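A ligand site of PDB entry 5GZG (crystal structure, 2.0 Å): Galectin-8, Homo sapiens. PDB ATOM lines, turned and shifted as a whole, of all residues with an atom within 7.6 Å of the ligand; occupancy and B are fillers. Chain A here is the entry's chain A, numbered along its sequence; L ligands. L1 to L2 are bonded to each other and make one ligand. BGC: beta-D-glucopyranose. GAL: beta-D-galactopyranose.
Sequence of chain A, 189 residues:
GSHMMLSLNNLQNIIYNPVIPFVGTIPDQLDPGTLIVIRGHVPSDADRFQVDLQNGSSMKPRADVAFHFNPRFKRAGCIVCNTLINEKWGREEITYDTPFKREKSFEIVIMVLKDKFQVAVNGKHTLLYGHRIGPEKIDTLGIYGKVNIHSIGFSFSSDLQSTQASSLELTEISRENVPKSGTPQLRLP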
ATOM      1  N   ARG A  48       0.145 -19.714  18.051  1.00  0.00           N
ATOM      2  CA  ARG A  48       0.782 -18.448  18.384  1.00  0.00           C
ATOM      3  C   ARG A  48       2.267 -18.514  18.064  1.00  0.00           C
ATOM      4  O   ARG A  48       2.859 -19.592  17.937  1.00  0.00           O
ATOM      5  CB  ARG A  48       0.587 -18.102  19.868  1.00  0.00           C
ATOM      6  CG  ARG A  48       1.067 -19.184  20.826  1.00  0.00           C
ATOM      7  CD  ARG A  48       0.947 -18.711  22.259  1.00  0.00           C
ATOM      8  NE  ARG A  48       2.206 -18.144  22.743  1.00  0.00           N
ATOM      9  CZ  ARG A  48       2.311 -17.392  23.846  1.00  0.00           C
ATOM     10  NH1 ARG A  48       1.244 -17.116  24.572  1.00  0.00           N
ATOM     11  NH2 ARG A  48       3.504 -16.944  24.214  1.00  0.00           N
ATOM     12  N   PHE A  49       2.881 -17.338  17.956  1.00  0.00           N
ATOM     13  CA  PHE A  49       4.335 -17.220  18.019  1.00  0.00           C
ATOM     14  C   PHE A  49       4.679 -15.908  18.718  1.00  0.00           C
ATOM     15  O   PHE A  49       3.806 -15.086  19.020  1.00  0.00           O
ATOM     16  CB  PHE A  49       4.997 -17.336  16.624  1.00  0.00           C
ATOM     17  CG  PHE A  49       4.828 -16.142  15.725  1.00  0.00           C
ATOM     18  CD1 PHE A  49       3.800 -16.090  14.792  1.00  0.00           C
ATOM     19  CD2 PHE A  49       5.742 -15.094  15.758  1.00  0.00           C
ATOM     20  CE1 PHE A  49       3.671 -15.000  13.947  1.00  0.00           C
ATOM     21  CE2 PHE A  49       5.602 -13.985  14.917  1.00  0.00           C
ATOM     22  CZ  PHE A  49       4.560 -13.954  14.017  1.00  0.00           C
ATOM     23  N   GLN A  50       5.966 -15.753  19.021  1.00  0.00           N
ATOM     24  CA  GLN A  50       6.417 -14.540  19.691  1.00  0.00           C
ATOM     25  C   GLN A  50       7.797 -14.127  19.222  1.00  0.00           C
ATOM     26  O   GLN A  50       8.653 -14.960  18.908  1.00  0.00           O
ATOM     27  CB  GLN A  50       6.412 -14.717  21.222  1.00  0.00           C
ATOM     28  CG  GLN A  50       7.296 -15.837  21.704  1.00  0.00           C
ATOM     29  CD  GLN A  50       6.863 -16.371  23.053  1.00  0.00           C
ATOM     30  OE1 GLN A  50       5.955 -17.196  23.127  1.00  0.00           O
ATOM     31  NE2 GLN A  50       7.503 -15.898  24.118  1.00  0.00           N
ATOM     32  N   ASP A  52      10.696 -11.914  21.080  1.00  0.00           N
ATOM     33  CA  ASP A  52      11.053 -11.404  22.405  1.00  0.00           C
ATOM     34  C   ASP A  52      12.364 -10.629  22.362  1.00  0.00           C
ATOM     35  O   ASP A  52      13.416 -11.192  22.032  1.00  0.00           O
ATOM     36  CB  ASP A  52      11.149 -12.535  23.409  1.00  0.00           C
ATOM     37  CG  ASP A  52       9.798 -13.158  23.750  1.00  0.00           C
ATOM     38  OD1 ASP A  52       8.729 -12.516  23.555  1.00  0.00           O
ATOM     39  OD2 ASP A  52       9.816 -14.294  24.270  1.00  0.00           O
ATOM     40  N   ARG A  62      14.423 -17.260  34.090  1.00  0.00           N
ATOM     41  CA  ARG A  62      14.136 -16.818  32.737  1.00  0.00           C
ATOM     42  C   ARG A  62      14.487 -15.338  32.560  1.00  0.00           C
ATOM     43  O   ARG A  62      14.068 -14.493  33.364  1.00  0.00           O
ATOM     44  CB  ARG A  62      12.675 -17.052  32.400  1.00  0.00           C
ATOM     45  CG  ARG A  62      12.319 -16.567  31.014  1.00  0.00           C
ATOM     46  CD  ARG A  62      10.885 -16.918  30.705  1.00  0.00           C
ATOM     47  NE  ARG A  62      10.494 -16.355  29.413  1.00  0.00           N
ATOM     48  CZ  ARG A  62       9.279 -16.466  28.918  1.00  0.00           C
ATOM     49  NH1 ARG A  62       8.329 -17.093  29.621  1.00  0.00           N
ATOM     50  NH2 ARG A  62       8.996 -15.930  27.729  1.00  0.00           N
ATOM     51  N   HIS A  68       7.775  -8.304  24.552  1.00  0.00           N
ATOM     52  CA  HIS A  68       7.139  -9.541  24.102  1.00  0.00           C
ATOM     53  C   HIS A  68       6.096  -9.171  23.051  1.00  0.00           C
ATOM     54  O   HIS A  68       5.084  -8.535  23.364  1.00  0.00           O
ATOM     55  CB  HIS A  68       6.512 -10.219  25.328  1.00  0.00           C
ATOM     56  CG  HIS A  68       5.685 -11.442  25.053  1.00  0.00           C
ATOM     57  ND1 HIS A  68       6.212 -12.604  24.532  1.00  0.00           N
ATOM     58  CD2 HIS A  68       4.390 -11.709  25.348  1.00  0.00           C
ATOM     59  CE1 HIS A  68       5.256 -13.516  24.467  1.00  0.00           C
ATOM     60  NE2 HIS A  68       4.135 -12.998  24.953  1.00  0.00           N
ATOM     61  N   ASN A  70       3.530 -10.818  20.530  1.00  0.00           N
ATOM     62  CA  ASN A  70       2.960 -12.172  20.545  1.00  0.00           C
ATOM     63  C   ASN A  70       1.675 -12.275  19.744  1.00  0.00           C
ATOM     64  O   ASN A  70       0.560 -12.147  20.301  1.00  0.00           O
ATOM     65  CB  ASN A  70       2.775 -12.610  22.001  1.00  0.00           C
ATOM     66  CG  ASN A  70       2.069 -13.946  22.125  1.00  0.00           C
ATOM     67  OD1 ASN A  70       1.241 -14.125  23.037  1.00  0.00           O
ATOM     68  ND2 ASN A  70       2.361 -14.886  21.226  1.00  0.00           N
ATOM     69  N   ARG A  72      -1.346 -14.203  18.186  1.00  0.00           N
ATOM     70  CA  ARG A  72      -2.143 -15.385  18.500  1.00  0.00           C
ATOM     71  C   ARG A  72      -3.242 -15.492  17.457  1.00  0.00           C
ATOM     72  O   ARG A  72      -3.784 -14.479  17.010  1.00  0.00           O
ATOM     73  CB  ARG A  72      -2.768 -15.285  19.898  1.00  0.00           C
ATOM     74  CG  ARG A  72      -1.772 -15.005  21.031  1.00  0.00           C
ATOM     75  CD  ARG A  72      -2.478 -14.874  22.392  1.00  0.00           C
ATOM     76  NE  ARG A  72      -1.499 -14.677  23.461  1.00  0.00           N
ATOM     77  CZ  ARG A  72      -1.786 -14.635  24.755  1.00  0.00           C
ATOM     78  NH1 ARG A  72      -3.047 -14.776  25.171  1.00  0.00           N
ATOM     79  NH2 ARG A  72      -0.814 -14.462  25.645  1.00  0.00           N
ATOM     80  N   CYS A  78      -5.220 -11.961  17.550  1.00  0.00           N
ATOM     81  CA  CYS A  78      -4.848 -10.698  18.169  1.00  0.00           C
ATOM     82  C   CYS A  78      -3.334 -10.663  18.284  1.00  0.00           C
ATOM     83  O   CYS A  78      -2.637 -11.614  17.894  1.00  0.00           O
ATOM     84  CB  CYS A  78      -5.478 -10.508  19.551  1.00  0.00           C
ATOM     85  SG  CYS A  78      -5.014 -11.758  20.760  1.00  0.00           S
ATOM     86  N   VAL A  80      -0.779  -9.850  21.526  1.00  0.00           N
ATOM     87  CA  VAL A  80      -0.507  -9.459  22.906  1.00  0.00           C
ATOM     88  C   VAL A  80       0.925  -8.941  22.975  1.00  0.00           C
ATOM     89  O   VAL A  80       1.859  -9.598  22.501  1.00  0.00           O
ATOM     90  CB  VAL A  80      -0.737 -10.643  23.856  1.00  0.00           C
ATOM     91  CG1 VAL A  80      -0.457 -10.250  25.290  1.00  0.00           C
ATOM     92  CG2 VAL A  80      -2.176 -11.163  23.734  1.00  0.00           C
ATOM     93  N   CYS A  81       1.108  -7.748  23.533  1.00  0.00           N
ATOM     94  CA  CYS A  81       2.421  -7.247  23.899  1.00  0.00           C
ATOM     95  C   CYS A  81       2.498  -7.085  25.405  1.00  0.00           C
ATOM     96  O   CYS A  81       1.494  -6.753  26.069  1.00  0.00           O
ATOM     97  CB  CYS A  81       2.730  -5.921  23.193  1.00  0.00           C
ATOM     98  SG  CYS A  81       2.771  -6.056  21.390  1.00  0.00           S
ATOM     99  N   ASN A  82       3.680  -7.328  25.967  1.00  0.00           N
ATOM    100  CA  ASN A  82       3.844  -7.349  27.415  1.00  0.00           C
ATOM    101  C   ASN A  82       5.338  -7.323  27.738  1.00  0.00           C
ATOM    102  O   ASN A  82       6.197  -7.351  26.846  1.00  0.00           O
ATOM    103  CB  ASN A  82       3.152  -8.575  28.029  1.00  0.00           C
ATOM    104  CG  ASN A  82       2.709  -8.335  29.465  1.00  0.00           C
ATOM    105  OD1 ASN A  82       3.132  -7.387  30.124  1.00  0.00           O
ATOM    106  ND2 ASN A  82       1.860  -9.228  29.958  1.00  0.00           N
ATOM    107  N   THR A  83       5.647  -7.251  29.029  1.00  0.00           N
ATOM    108  CA  THR A  83       7.015  -7.225  29.536  1.00  0.00           C
ATOM    109  C   THR A  83       7.109  -8.223  30.681  1.00  0.00           C
ATOM    110  O   THR A  83       6.226  -8.278  31.535  1.00  0.00           O
ATOM    111  CB  THR A  83       7.381  -5.823  30.045  1.00  0.00           C
ATOM    112  OG1 THR A  83       7.525  -4.932  28.936  1.00  0.00           O
ATOM    113  CG2 THR A  83       8.662  -5.852  30.858  1.00  0.00           C
ATOM    114  N   LEU A  84       8.170  -9.020  30.674  1.00  0.00           N
ATOM    115  CA  LEU A  84       8.442 -10.012  31.707  1.00  0.00           C
ATOM    116  C   LEU A  84       9.618  -9.558  32.555  1.00  0.00           C
ATOM    117  O   LEU A  84      10.690  -9.257  32.014  1.00  0.00           O
ATOM    118  CB  LEU A  84       8.733 -11.380  31.082  1.00  0.00           C
ATOM    119  CG  LEU A  84       9.023 -12.541  32.037  1.00  0.00           C
ATOM    120  CD1 LEU A  84       7.736 -13.115  32.603  1.00  0.00           C
ATOM    121  CD2 LEU A  84       9.830 -13.617  31.353  1.00  0.00           C
ATOM    122  N   TRP A  89       4.849 -11.680  34.354  1.00  0.00           N
ATOM    123  CA  TRP A  89       4.298 -10.838  33.292  1.00  0.00           C
ATOM    124  C   TRP A  89       3.643  -9.588  33.866  1.00  0.00           C
ATOM    125  O   TRP A  89       3.063  -9.589  34.960  1.00  0.00           O
ATOM    126  CB  TRP A  89       3.292 -11.636  32.466  1.00  0.00           C
ATOM    127  CG  TRP A  89       3.970 -12.637  31.586  1.00  0.00           C
ATOM    128  CD1 TRP A  89       3.951 -14.005  31.696  1.00  0.00           C
ATOM    129  CD2 TRP A  89       4.789 -12.341  30.452  1.00  0.00           C
ATOM    130  NE1 TRP A  89       4.722 -14.566  30.685  1.00  0.00           N
ATOM    131  CE2 TRP A  89       5.232 -13.572  29.915  1.00  0.00           C
ATOM    132  CE3 TRP A  89       5.183 -11.155  29.836  1.00  0.00           C
ATOM    133  CZ2 TRP A  89       6.069 -13.636  28.797  1.00  0.00           C
ATOM    134  CZ3 TRP A  89       6.003 -11.221  28.728  1.00  0.00           C
ATOM    135  CH2 TRP A  89       6.430 -12.452  28.222  1.00  0.00           C
ATOM    136  N   GLY A  90       3.707  -8.498  33.097  1.00  0.00           N
ATOM    137  CA  GLY A  90       3.073  -7.250  33.464  1.00  0.00           C
ATOM    138  C   GLY A  90       1.707  -7.086  32.827  1.00  0.00           C
ATOM    139  O   GLY A  90       1.052  -8.063  32.449  1.00  0.00           O
ATOM    140  N   ARG A  91       1.276  -5.815  32.701  1.00  0.00           N
ATOM    141  CA  ARG A  91      -0.012  -5.472  32.110  1.00  0.00           C
ATOM    142  C   ARG A  91      -0.002  -5.696  30.605  1.00  0.00           C
ATOM    143  O   ARG A  91       0.852  -5.129  29.903  1.00  0.00           O
ATOM    144  CB  ARG A  91      -0.342  -4.013  32.395  1.00  0.00           C
ATOM    145  CG  ARG A  91      -1.734  -3.588  31.960  1.00  0.00           C
ATOM    146  CD  ARG A  91      -1.704  -2.507  30.866  1.00  0.00           C
ATOM    147  NE  ARG A  91      -3.075  -2.220  30.464  1.00  0.00           N
ATOM    148  CZ  ARG A  91      -3.436  -1.479  29.418  1.00  0.00           C
ATOM    149  NH1 ARG A  91      -2.528  -0.917  28.629  1.00  0.00           N
ATOM    150  NH2 ARG A  91      -4.725  -1.311  29.163  1.00  0.00           N
ATOM    151  N   GLU A  92      -0.960  -6.485  30.107  1.00  0.00           N
ATOM    152  CA  GLU A  92      -1.066  -6.770  28.672  1.00  0.00           C
ATOM    153  C   GLU A  92      -1.606  -5.591  27.867  1.00  0.00           C
ATOM    154  O   GLU A  92      -2.570  -4.938  28.267  1.00  0.00           O
ATOM    155  CB  GLU A  92      -1.976  -7.961  28.418  1.00  0.00           C
ATOM    156  CG  GLU A  92      -1.417  -9.275  28.866  1.00  0.00           C
ATOM    157  CD  GLU A  92      -2.272 -10.434  28.430  1.00  0.00           C
ATOM    158  OE1 GLU A  92      -3.454 -10.207  28.087  1.00  0.00           O
ATOM    159  OE2 GLU A  92      -1.743 -11.557  28.387  1.00  0.00           O
ATOM    160  N   GLU A  93      -0.988  -5.325  26.721  1.00  0.00           N
ATOM    161  CA  GLU A  93      -1.481  -4.355  25.744  1.00  0.00           C
ATOM    162  C   GLU A  93      -1.918  -5.173  24.533  1.00  0.00           C
ATOM    163  O   GLU A  93      -1.082  -5.674  23.769  1.00  0.00           O
ATOM    164  CB  GLU A  93      -0.409  -3.328  25.380  1.00  0.00           C
ATOM    165  CG  GLU A  93       0.172  -2.647  26.579  1.00  0.00           C
ATOM    166  CD  GLU A  93       1.129  -1.551  26.228  1.00  0.00           C
ATOM    167  OE1 GLU A  93       1.078  -1.031  25.083  1.00  0.00           O
ATOM    168  OE2 GLU A  93       1.953  -1.212  27.109  1.00  0.00           O
ATOM    169  N   ILE A  94      -3.225  -5.328  24.356  1.00  0.00           N
ATOM    170  CA  ILE A  94      -3.768  -6.213  23.335  1.00  0.00           C
ATOM    171  C   ILE A  94      -4.222  -5.374  22.139  1.00  0.00           C
ATOM    172  O   ILE A  94      -4.968  -4.401  22.302  1.00  0.00           O
ATOM    173  CB  ILE A  94      -4.928  -7.066  23.896  1.00  0.00           C
ATOM    174  CG1 ILE A  94      -4.418  -7.941  25.041  1.00  0.00           C
ATOM    175  CG2 ILE A  94      -5.504  -7.955  22.813  1.00  0.00           C
ATOM    176  CD1 ILE A  94      -5.481  -8.873  25.599  1.00  0.00           C
ATOM    177  N   TYR A  96      -6.257  -5.826  18.672  1.00  0.00           N
ATOM    178  CA  TYR A  96      -7.153  -6.801  18.050  1.00  0.00           C
ATOM    179  C   TYR A  96      -7.128  -6.773  16.530  1.00  0.00           C
ATOM    180  O   TYR A  96      -7.511  -7.756  15.897  1.00  0.00           O
ATOM    181  CB  TYR A  96      -8.578  -6.605  18.579  1.00  0.00           C
ATOM    182  CG  TYR A  96      -8.738  -7.081  20.012  1.00  0.00           C
ATOM    183  CD1 TYR A  96      -8.866  -8.436  20.297  1.00  0.00           C
ATOM    184  CD2 TYR A  96      -8.701  -6.195  21.075  1.00  0.00           C
ATOM    185  CE1 TYR A  96      -8.999  -8.891  21.598  1.00  0.00           C
ATOM    186  CE2 TYR A  96      -8.822  -6.639  22.380  1.00  0.00           C
ATOM    187  CZ  TYR A  96      -8.965  -7.996  22.639  1.00  0.00           C
ATOM    188  OH  TYR A  96      -9.089  -8.451  23.935  1.00  0.00           O
HETATM  189  C2  BGC L   1      -4.259 -13.669  29.178  1.00  0.00           C
HETATM  190  C3  BGC L   1      -3.143 -14.499  28.672  1.00  0.00           C
HETATM  191  C4  BGC L   1      -2.196 -14.919  29.688  1.00  0.00           C
HETATM  192  C5  BGC L   1      -2.909 -15.587  30.824  1.00  0.00           C
HETATM  193  C6  BGC L   1      -2.179 -15.391  32.147  1.00  0.00           C
HETATM  194  C1  BGC L   1      -5.132 -14.639  29.943  1.00  0.00           C
HETATM  195  O1  BGC L   1      -6.199 -13.987  30.343  1.00  0.00           O
HETATM  196  O2  BGC L   1      -5.052 -13.062  28.120  1.00  0.00           O
HETATM  197  O3  BGC L   1      -2.490 -13.818  27.534  1.00  0.00           O
HETATM  198  O4  BGC L   1      -1.199 -15.895  29.029  1.00  0.00           O
HETATM  199  O5  BGC L   1      -4.271 -15.096  31.125  1.00  0.00           O
HETATM  200  O6  BGC L   1      -0.790 -15.585  32.004  1.00  0.00           O
HETATM  201  C1  GAL L   2       0.150 -15.487  29.015  1.00  0.00           C
HETATM  202  C2  GAL L   2       1.064 -16.511  28.325  1.00  0.00           C
HETATM  203  C3  GAL L   2       2.473 -16.081  28.115  1.00  0.00           C
HETATM  204  C4  GAL L   2       2.657 -14.661  27.714  1.00  0.00           C
HETATM  205  C5  GAL L   2       1.728 -13.688  28.450  1.00  0.00           C
HETATM  206  C6  GAL L   2       1.753 -12.308  27.842  1.00  0.00           C
HETATM  207  O2  GAL L   2       1.088 -17.805  28.992  1.00  0.00           O
HETATM  208  O3  GAL L   2       3.055 -16.983  27.143  1.00  0.00           O
HETATM  209  O4  GAL L   2       2.341 -14.625  26.304  1.00  0.00           O
HETATM  210  O5  GAL L   2       0.325 -14.162  28.419  1.00  0.00           O
HETATM  211  O6  GAL L   2       1.104 -11.415  28.714  1.00  0.00           O
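CG1 of Val 80 touches O6 of GAL L2, at 3.9 Å.
CE2 of Trp 89 touches C4 of GAL L2, 3.6 Å away.
Of the 21 residues printed, 8 come within 4 Å of the ligand.
OE2 of Glu 92 is in hydrogen-bond range of O3 of BGC L1, at 2.5 Å.
The guanidinium group of Arg 72 is in hydrogen-bond range of an oxygen (O3) of BGC L1 (2.6 Å).
The side-chain amide nitrogen (ND2) of Asn 82 sits at hydrogen-bond distance from an oxygen (O6) of GAL L2.
NE2 of His 68 is in hydrogen-bond range of O4 of GAL L2 (2.8 Å).
The side-chain amide oxygen (OD1) of Asn 70 sits at hydrogen-bond distance from an oxygen (O4) of GAL L2 (3.5 Å).
O3 of GAL L2 lies within hydrogen-bond range of NH2 of Arg 48 (3.0 Å).
The side-chain amide oxygen (OD1) of Asn 82 sits close to the backbone carbonyl oxygen (O) of Arg 91.
The backbone NH (N) of Asn 70 is in hydrogen-bond range of the backbone carbonyl oxygen (O) of Val 80.
The side-chain amide nitrogen (ND2) of Asn 70 lies within hydrogen-bond range of the backbone carbonyl oxygen (O) of Phe 49.
ND1 of His 68 lies within hydrogen-bond range of OD1 of Asp 52, 2.7 Å away.
O of Asn 82 is in hydrogen-bond range of N of His 68.
NH1 of Arg 48 sits at hydrogen-bond distance from OD1 of Asn 70 (3.4 Å).
The guanidinium group (NE) of Arg 72 lies within hydrogen-bond range of the side-chain amide oxygen (OD1) of Asn 70 (2.8 Å).
O of Gly 90 lies within hydrogen-bond range of ND2 of Asn 82 (2.9 Å).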
